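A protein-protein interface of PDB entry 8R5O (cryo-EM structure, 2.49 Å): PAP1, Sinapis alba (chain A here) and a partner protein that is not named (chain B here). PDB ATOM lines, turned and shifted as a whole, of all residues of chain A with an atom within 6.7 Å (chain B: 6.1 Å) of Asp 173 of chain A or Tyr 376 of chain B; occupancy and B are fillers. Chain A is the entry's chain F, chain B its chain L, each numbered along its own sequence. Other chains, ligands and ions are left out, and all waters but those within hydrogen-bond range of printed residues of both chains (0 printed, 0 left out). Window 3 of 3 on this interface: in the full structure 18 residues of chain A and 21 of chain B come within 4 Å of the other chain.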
ATOM      1  N   PRO A 141     -11.586 -16.516 -12.318  1.00  0.00           N
ATOM      2  CA  PRO A 141     -11.115 -17.254 -11.134  1.00  0.00           C
ATOM      3  C   PRO A 141     -10.695 -16.337 -10.003  1.00  0.00           C
ATOM      4  O   PRO A 141     -10.898 -16.667  -8.829  1.00  0.00           O
ATOM      5  CB  PRO A 141      -9.932 -18.068 -11.677  1.00  0.00           C
ATOM      6  CG  PRO A 141     -10.178 -18.169 -13.142  1.00  0.00           C
ATOM      7  CD  PRO A 141     -10.840 -16.884 -13.533  1.00  0.00           C
ATOM      8  N   ILE A 145     -12.119 -15.961  -5.975  1.00  0.00           N
ATOM      9  CA  ILE A 145     -11.186 -15.944  -4.854  1.00  0.00           C
ATOM     10  C   ILE A 145     -11.422 -14.727  -3.967  1.00  0.00           C
ATOM     11  O   ILE A 145     -11.276 -14.806  -2.741  1.00  0.00           O
ATOM     12  CB  ILE A 145      -9.739 -16.004  -5.377  1.00  0.00           C
ATOM     13  CG1 ILE A 145      -9.468 -17.366  -6.014  1.00  0.00           C
ATOM     14  CG2 ILE A 145      -8.745 -15.748  -4.263  1.00  0.00           C
ATOM     15  CD1 ILE A 145      -8.062 -17.526  -6.531  1.00  0.00           C
ATOM     16  N   MET A 167     -16.765 -22.815  -8.115  1.00  0.00           N
ATOM     17  CA  MET A 167     -15.525 -22.835  -8.887  1.00  0.00           C
ATOM     18  C   MET A 167     -15.277 -24.207  -9.500  1.00  0.00           C
ATOM     19  O   MET A 167     -14.819 -24.310 -10.644  1.00  0.00           O
ATOM     20  CB  MET A 167     -14.347 -22.427  -8.005  1.00  0.00           C
ATOM     21  CG  MET A 167     -14.515 -21.077  -7.340  1.00  0.00           C
ATOM     22  SD  MET A 167     -13.082 -20.589  -6.364  1.00  0.00           S
ATOM     23  CE  MET A 167     -11.846 -20.423  -7.646  1.00  0.00           C
ATOM     24  N   GLU A 168     -15.560 -25.274  -8.749  1.00  0.00           N
ATOM     25  CA  GLU A 168     -15.468 -26.617  -9.308  1.00  0.00           C
ATOM     26  C   GLU A 168     -16.464 -26.799 -10.446  1.00  0.00           C
ATOM     27  O   GLU A 168     -16.146 -27.416 -11.469  1.00  0.00           O
ATOM     28  CB  GLU A 168     -15.701 -27.657  -8.211  1.00  0.00           C
ATOM     29  CG  GLU A 168     -14.992 -28.990  -8.431  1.00  0.00           C
ATOM     30  CD  GLU A 168     -15.694 -29.883  -9.438  1.00  0.00           C
ATOM     31  OE1 GLU A 168     -16.893 -29.662  -9.707  1.00  0.00           O
ATOM     32  OE2 GLU A 168     -15.042 -30.814  -9.959  1.00  0.00           O
ATOM     33  N   ASN A 171     -15.328 -25.337 -13.460  1.00  0.00           N
ATOM     34  CA  ASN A 171     -14.142 -26.062 -13.909  1.00  0.00           C
ATOM     35  C   ASN A 171     -12.842 -25.342 -13.574  1.00  0.00           C
ATOM     36  O   ASN A 171     -11.820 -25.581 -14.223  1.00  0.00           O
ATOM     37  CB  ASN A 171     -14.200 -26.360 -15.412  1.00  0.00           C
ATOM     38  CG  ASN A 171     -15.383 -27.225 -15.787  1.00  0.00           C
ATOM     39  OD1 ASN A 171     -15.331 -28.450 -15.672  1.00  0.00           O
ATOM     40  ND2 ASN A 171     -16.457 -26.594 -16.241  1.00  0.00           N
ATOM     41  N   TYR A 172     -12.849 -24.464 -12.575  1.00  0.00           N
ATOM     42  CA  TYR A 172     -11.621 -23.836 -12.118  1.00  0.00           C
ATOM     43  C   TYR A 172     -10.850 -24.792 -11.211  1.00  0.00           C
ATOM     44  O   TYR A 172     -11.256 -25.933 -10.972  1.00  0.00           O
ATOM     45  CB  TYR A 172     -11.923 -22.525 -11.397  1.00  0.00           C
ATOM     46  CG  TYR A 172     -12.434 -21.424 -12.297  1.00  0.00           C
ATOM     47  CD1 TYR A 172     -12.126 -21.408 -13.649  1.00  0.00           C
ATOM     48  CD2 TYR A 172     -13.221 -20.399 -11.792  1.00  0.00           C
ATOM     49  CE1 TYR A 172     -12.592 -20.402 -14.475  1.00  0.00           C
ATOM     50  CE2 TYR A 172     -13.690 -19.391 -12.608  1.00  0.00           C
ATOM     51  CZ  TYR A 172     -13.373 -19.397 -13.948  1.00  0.00           C
ATOM     52  OH  TYR A 172     -13.838 -18.393 -14.765  1.00  0.00           O
ATOM     53  N   ASP A 173      -9.722 -24.318 -10.690  1.00  0.00           N
ATOM     54  CA  ASP A 173      -8.884 -25.089  -9.776  1.00  0.00           C
ATOM     55  C   ASP A 173      -9.083 -24.524  -8.376  1.00  0.00           C
ATOM     56  O   ASP A 173      -8.643 -23.408  -8.081  1.00  0.00           O
ATOM     57  CB  ASP A 173      -7.419 -25.030 -10.199  1.00  0.00           C
ATOM     58  CG  ASP A 173      -6.540 -25.959  -9.386  1.00  0.00           C
ATOM     59  OD1 ASP A 173      -6.691 -27.191  -9.520  1.00  0.00           O
ATOM     60  OD2 ASP A 173      -5.697 -25.457  -8.612  1.00  0.00           O
ATOM     61  N   ILE A 174      -9.744 -25.300  -7.511  1.00  0.00           N
ATOM     62  CA  ILE A 174     -10.150 -24.805  -6.200  1.00  0.00           C
ATOM     63  C   ILE A 174      -9.084 -24.993  -5.132  1.00  0.00           C
ATOM     64  O   ILE A 174      -9.313 -24.608  -3.978  1.00  0.00           O
ATOM     65  CB  ILE A 174     -11.448 -25.489  -5.727  1.00  0.00           C
ATOM     66  CG1 ILE A 174     -11.190 -26.968  -5.436  1.00  0.00           C
ATOM     67  CG2 ILE A 174     -12.536 -25.336  -6.769  1.00  0.00           C
ATOM     68  CD1 ILE A 174     -12.351 -27.664  -4.768  1.00  0.00           C
ATOM     69  N   ARG A 175      -7.933 -25.581  -5.468  1.00  0.00           N
ATOM     70  CA  ARG A 175      -6.911 -25.815  -4.452  1.00  0.00           C
ATOM     71  C   ARG A 175      -6.412 -24.505  -3.857  1.00  0.00           C
ATOM     72  O   ARG A 175      -6.312 -24.364  -2.634  1.00  0.00           O
ATOM     73  CB  ARG A 175      -5.745 -26.611  -5.037  1.00  0.00           C
ATOM     74  CG  ARG A 175      -4.563 -26.710  -4.083  1.00  0.00           C
ATOM     75  CD  ARG A 175      -3.493 -27.661  -4.578  1.00  0.00           C
ATOM     76  NE  ARG A 175      -2.446 -27.847  -3.581  1.00  0.00           N
ATOM     77  CZ  ARG A 175      -1.299 -27.181  -3.563  1.00  0.00           C
ATOM     78  NH1 ARG A 175      -1.006 -26.286  -4.491  1.00  0.00           N
ATOM     79  NH2 ARG A 175      -0.425 -27.422  -2.591  1.00  0.00           N
ATOM     80  N   GLN A 176      -6.100 -23.529  -4.711  1.00  0.00           N
ATOM     81  CA  GLN A 176      -5.579 -22.260  -4.215  1.00  0.00           C
ATOM     82  C   GLN A 176      -6.636 -21.493  -3.428  1.00  0.00           C
ATOM     83  O   GLN A 176      -6.327 -20.873  -2.405  1.00  0.00           O
ATOM     84  CB  GLN A 176      -5.051 -21.420  -5.375  1.00  0.00           C
ATOM     85  CG  GLN A 176      -4.557 -20.046  -4.966  1.00  0.00           C
ATOM     86  CD  GLN A 176      -3.818 -19.339  -6.081  1.00  0.00           C
ATOM     87  OE1 GLN A 176      -3.124 -19.969  -6.877  1.00  0.00           O
ATOM     88  NE2 GLN A 176      -3.965 -18.021  -6.146  1.00  0.00           N
ATOM     89  N   ALA A 177      -7.889 -21.519  -3.892  1.00  0.00           N
ATOM     90  CA  ALA A 177      -8.953 -20.834  -3.167  1.00  0.00           C
ATOM     91  C   ALA A 177      -9.275 -21.532  -1.853  1.00  0.00           C
ATOM     92  O   ALA A 177      -9.632 -20.870  -0.873  1.00  0.00           O
ATOM     93  CB  ALA A 177     -10.204 -20.737  -4.037  1.00  0.00           C
ATOM     94  N   TRP A 178      -9.160 -22.860  -1.814  1.00  0.00           N
ATOM     95  CA  TRP A 178      -9.353 -23.585  -0.563  1.00  0.00           C
ATOM     96  C   TRP A 178      -8.262 -23.247   0.446  1.00  0.00           C
ATOM     97  O   TRP A 178      -8.538 -23.118   1.644  1.00  0.00           O
ATOM     98  CB  TRP A 178      -9.400 -25.087  -0.834  1.00  0.00           C
ATOM     99  CG  TRP A 178      -9.322 -25.926   0.396  1.00  0.00           C
ATOM    100  CD1 TRP A 178     -10.299 -26.111   1.325  1.00  0.00           C
ATOM    101  CD2 TRP A 178      -8.204 -26.710   0.826  1.00  0.00           C
ATOM    102  NE1 TRP A 178      -9.859 -26.957   2.313  1.00  0.00           N
ATOM    103  CE2 TRP A 178      -8.575 -27.340   2.029  1.00  0.00           C
ATOM    104  CE3 TRP A 178      -6.925 -26.939   0.310  1.00  0.00           C
ATOM    105  CZ2 TRP A 178      -7.713 -28.183   2.724  1.00  0.00           C
ATOM    106  CZ3 TRP A 178      -6.071 -27.775   1.003  1.00  0.00           C
ATOM    107  CH2 TRP A 178      -6.469 -28.388   2.196  1.00  0.00           C
ATOM    108  N   ASN B 367      -4.821 -18.785 -18.353  1.00  0.00           N
ATOM    109  CA  ASN B 367      -5.310 -19.979 -17.659  1.00  0.00           C
ATOM    110  C   ASN B 367      -4.174 -20.762 -17.006  1.00  0.00           C
ATOM    111  O   ASN B 367      -4.138 -21.992 -17.052  1.00  0.00           O
ATOM    112  CB  ASN B 367      -6.111 -20.883 -18.600  1.00  0.00           C
ATOM    113  CG  ASN B 367      -7.324 -20.192 -19.179  1.00  0.00           C
ATOM    114  OD1 ASN B 367      -7.914 -19.314 -18.552  1.00  0.00           O
ATOM    115  ND2 ASN B 367      -7.705 -20.586 -20.387  1.00  0.00           N
ATOM    116  N   ILE B 368      -3.236 -20.049 -16.396  1.00  0.00           N
ATOM    117  CA  ILE B 368      -2.164 -20.678 -15.636  1.00  0.00           C
ATOM    118  C   ILE B 368      -2.606 -20.753 -14.181  1.00  0.00           C
ATOM    119  O   ILE B 368      -2.815 -19.723 -13.532  1.00  0.00           O
ATOM    120  CB  ILE B 368      -0.847 -19.905 -15.779  1.00  0.00           C
ATOM    121  CG1 ILE B 368      -0.454 -19.798 -17.251  1.00  0.00           C
ATOM    122  CG2 ILE B 368       0.258 -20.593 -14.994  1.00  0.00           C
ATOM    123  CD1 ILE B 368       0.780 -18.973 -17.488  1.00  0.00           C
ATOM    124  N   PHE B 369      -2.751 -21.968 -13.672  1.00  0.00           N
ATOM    125  CA  PHE B 369      -3.269 -22.213 -12.334  1.00  0.00           C
ATOM    126  C   PHE B 369      -2.188 -22.845 -11.466  1.00  0.00           C
ATOM    127  O   PHE B 369      -1.092 -23.166 -11.927  1.00  0.00           O
ATOM    128  CB  PHE B 369      -4.515 -23.099 -12.390  1.00  0.00           C
ATOM    129  CG  PHE B 369      -5.658 -22.483 -13.136  1.00  0.00           C
ATOM    130  CD1 PHE B 369      -6.430 -21.496 -12.550  1.00  0.00           C
ATOM    131  CD2 PHE B 369      -5.960 -22.887 -14.423  1.00  0.00           C
ATOM    132  CE1 PHE B 369      -7.482 -20.923 -13.233  1.00  0.00           C
ATOM    133  CE2 PHE B 369      -7.012 -22.319 -15.111  1.00  0.00           C
ATOM    134  CZ  PHE B 369      -7.773 -21.336 -14.516  1.00  0.00           C
ATOM    135  N   GLY B 370      -2.514 -23.018 -10.190  1.00  0.00           N
ATOM    136  CA  GLY B 370      -1.591 -23.597  -9.240  1.00  0.00           C
ATOM    137  C   GLY B 370      -0.704 -22.565  -8.584  1.00  0.00           C
ATOM    138  O   GLY B 370      -0.717 -21.372  -8.901  1.00  0.00           O
ATOM    139  N   LEU B 371       0.084 -23.046  -7.634  1.00  0.00           N
ATOM    140  CA  LEU B 371       1.046 -22.216  -6.935  1.00  0.00           C
ATOM    141  C   LEU B 371       2.241 -21.922  -7.839  1.00  0.00           C
ATOM    142  O   LEU B 371       2.468 -22.624  -8.826  1.00  0.00           O
ATOM    143  CB  LEU B 371       1.491 -22.913  -5.653  1.00  0.00           C
ATOM    144  CG  LEU B 371       0.385 -23.180  -4.629  1.00  0.00           C
ATOM    145  CD1 LEU B 371       0.965 -23.760  -3.353  1.00  0.00           C
ATOM    146  CD2 LEU B 371      -0.398 -21.909  -4.336  1.00  0.00           C
ATOM    147  N   GLU B 374       4.399 -24.723  -8.905  1.00  0.00           N
ATOM    148  CA  GLU B 374       3.711 -25.808  -9.594  1.00  0.00           C
ATOM    149  C   GLU B 374       2.734 -25.253 -10.621  1.00  0.00           C
ATOM    150  O   GLU B 374       1.606 -25.736 -10.757  1.00  0.00           O
ATOM    151  CB  GLU B 374       2.994 -26.726  -8.602  1.00  0.00           C
ATOM    152  CG  GLU B 374       3.939 -27.482  -7.676  1.00  0.00           C
ATOM    153  CD  GLU B 374       3.225 -28.469  -6.773  1.00  0.00           C
ATOM    154  OE1 GLU B 374       1.977 -28.482  -6.768  1.00  0.00           O
ATOM    155  OE2 GLU B 374       3.917 -29.234  -6.069  1.00  0.00           O
ATOM    156  N   TYR B 375       3.158 -24.224 -11.353  1.00  0.00           N
ATOM    157  CA  TYR B 375       2.326 -23.649 -12.400  1.00  0.00           C
ATOM    158  C   TYR B 375       2.033 -24.678 -13.483  1.00  0.00           C
ATOM    159  O   TYR B 375       2.894 -25.479 -13.855  1.00  0.00           O
ATOM    160  CB  TYR B 375       3.018 -22.441 -13.025  1.00  0.00           C
ATOM    161  CG  TYR B 375       2.877 -21.150 -12.262  1.00  0.00           C
ATOM    162  CD1 TYR B 375       1.760 -20.897 -11.478  1.00  0.00           C
ATOM    163  CD2 TYR B 375       3.856 -20.174 -12.338  1.00  0.00           C
ATOM    164  CE1 TYR B 375       1.631 -19.707 -10.787  1.00  0.00           C
ATOM    165  CE2 TYR B 375       3.737 -18.987 -11.654  1.00  0.00           C
ATOM    166  CZ  TYR B 375       2.625 -18.757 -10.880  1.00  0.00           C
ATOM    167  OH  TYR B 375       2.517 -17.569 -10.198  1.00  0.00           O
ATOM    168  N   TYR B 376       0.808 -24.647 -14.000  1.00  0.00           N
ATOM    169  CA  TYR B 376       0.427 -25.523 -15.096  1.00  0.00           C
ATOM    170  C   TYR B 376      -0.635 -24.830 -15.934  1.00  0.00           C
ATOM    171  O   TYR B 376      -1.292 -23.888 -15.487  1.00  0.00           O
ATOM    172  CB  TYR B 376      -0.078 -26.878 -14.588  1.00  0.00           C
ATOM    173  CG  TYR B 376      -1.457 -26.832 -13.972  1.00  0.00           C
ATOM    174  CD1 TYR B 376      -1.649 -26.350 -12.685  1.00  0.00           C
ATOM    175  CD2 TYR B 376      -2.565 -27.275 -14.677  1.00  0.00           C
ATOM    176  CE1 TYR B 376      -2.906 -26.306 -12.120  1.00  0.00           C
ATOM    177  CE2 TYR B 376      -3.827 -27.234 -14.121  1.00  0.00           C
ATOM    178  CZ  TYR B 376      -3.992 -26.750 -12.842  1.00  0.00           C
ATOM    179  OH  TYR B 376      -5.249 -26.710 -12.286  1.00  0.00           O
ATOM    180  N   HIS B 377      -0.789 -25.303 -17.166  1.00  0.00           N
ATOM    181  CA  HIS B 377      -1.781 -24.774 -18.089  1.00  0.00           C
ATOM    182  C   HIS B 377      -2.967 -25.727 -18.156  1.00  0.00           C
ATOM    183  O   HIS B 377      -2.786 -26.940 -18.303  1.00  0.00           O
ATOM    184  CB  HIS B 377      -1.186 -24.573 -19.483  1.00  0.00           C
ATOM    185  CG  HIS B 377      -2.181 -24.107 -20.500  1.00  0.00           C
ATOM    186  ND1 HIS B 377      -2.955 -22.980 -20.321  1.00  0.00           N
ATOM    187  CD2 HIS B 377      -2.531 -24.615 -21.704  1.00  0.00           C
ATOM    188  CE1 HIS B 377      -3.738 -22.815 -21.371  1.00  0.00           C
ATOM    189  NE2 HIS B 377      -3.501 -23.794 -22.225  1.00  0.00           N
ATOM    190  N   ASP B 378      -4.170 -25.176 -18.050  1.00  0.00           N
ATOM    191  CA  ASP B 378      -5.379 -25.988 -18.048  1.00  0.00           C
ATOM    192  C   ASP B 378      -5.639 -26.589 -19.427  1.00  0.00           C
ATOM    193  O   ASP B 378      -6.438 -26.068 -20.205  1.00  0.00           O
ATOM    194  CB  ASP B 378      -6.580 -25.157 -17.596  1.00  0.00           C
ATOM    195  CG  ASP B 378      -7.586 -25.972 -16.811  1.00  0.00           C
ATOM    196  OD1 ASP B 378      -7.612 -27.207 -16.984  1.00  0.00           O
ATOM    197  OD2 ASP B 378      -8.348 -25.379 -16.017  1.00  0.00           O
ATOM    198  N   ILE B 393       4.507 -20.034 -19.084  1.00  0.00           N
ATOM    199  CA  ILE B 393       4.693 -20.330 -17.667  1.00  0.00           C
ATOM    200  C   ILE B 393       6.015 -19.756 -17.181  1.00  0.00           C
ATOM    201  O   ILE B 393       6.092 -19.147 -16.107  1.00  0.00           O
ATOM    202  CB  ILE B 393       4.610 -21.847 -17.420  1.00  0.00           C
ATOM    203  CG1 ILE B 393       3.187 -22.350 -17.662  1.00  0.00           C
ATOM    204  CG2 ILE B 393       5.076 -22.186 -16.015  1.00  0.00           C
ATOM    205  CD1 ILE B 393       3.024 -23.831 -17.436  1.00  0.00           C
ATOM    206  N   ARG B 397       6.868 -16.646 -14.287  1.00  0.00           N
ATOM    207  CA  ARG B 397       7.845 -16.713 -13.208  1.00  0.00           C
ATOM    208  C   ARG B 397       8.961 -15.686 -13.355  1.00  0.00           C
ATOM    209  O   ARG B 397       9.548 -15.277 -12.348  1.00  0.00           O
ATOM    210  CB  ARG B 397       8.437 -18.119 -13.132  1.00  0.00           C
ATOM    211  CG  ARG B 397       7.454 -19.170 -12.663  1.00  0.00           C
ATOM    212  CD  ARG B 397       7.917 -20.560 -13.035  1.00  0.00           C
ATOM    213  NE  ARG B 397       7.088 -21.586 -12.419  1.00  0.00           N
ATOM    214  CZ  ARG B 397       7.024 -22.842 -12.834  1.00  0.00           C
ATOM    215  NH1 ARG B 397       7.714 -23.260 -13.880  1.00  0.00           N
ATOM    216  NH2 ARG B 397       6.240 -23.699 -12.186  1.00  0.00           N
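The backbone carbonyl oxygen of Asn 367 of chain B sits at hydrogen-bond distance from the backbone NH of Asp 378 of chain B.
N of Phe 369 of chain B lies within hydrogen-bond range of O of Tyr 376 of chain B, at 3.0 Å.
Asp 173 of chain A touches one residue of chain B.
Printed residues of chain B within 4 Å of Gln 176 of chain A: Gly 370.
Of the printed residues of chain A, Gly 370 of chain B touches Gln 176 (3.4 Å).
Of the printed residues of chain B, Pro 141 of chain A touches Phe 369.
Of the printed residues of chain B, Asn 171 of chain A touches Asp 378.
Printed residues of chain A within 4 Å of Asp 378 of chain B: Asn 171 (3.9 Å).
Ile 174 of chain A touches none of the printed residues of chain B.
Arg 397 of chain B touches none of the printed residues of chain A.
The nearest printed residue of chain B that does not touch Arg 175 of chain A is Glu 374 of chain B (4.3 Å).
OH of Tyr 376 of chain B is in hydrogen-bond range of OD1 of Asp 173 of chain A (3.2 Å).
The backbone carbonyl oxygen (O) of Gly 370 of chain B lies close to the side-chain amide oxygen (OE1) of Gln 176 of chain A (3.4 Å).
Among the printed residues, pairs that only touch across the chains: Arg 175 of chain A with Leu 371 of chain B (3.4 Å), Pro 141 of chain A with Phe 369 of chain B (3.9 Å) and Asn 171 of chain A with Asp 378 of chain B (3.9 Å).
Of the 12 printed residues of chain A, 5 touch a printed residue of chain B.
Printed residues of chain B that touch a printed residue of chain A: Phe 369, Gly 370, Leu 371, Tyr 376 and Asp 378.
Hydrophobic or aromatic side chains of chain B within 4 Å of the printed part of chain A: Phe 369, Leu 371 and Tyr 376.
Among the printed residues, no Asp or Glu carboxylate lies within 4 Å of a Lys or Arg side-chain nitrogen of the other chain.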
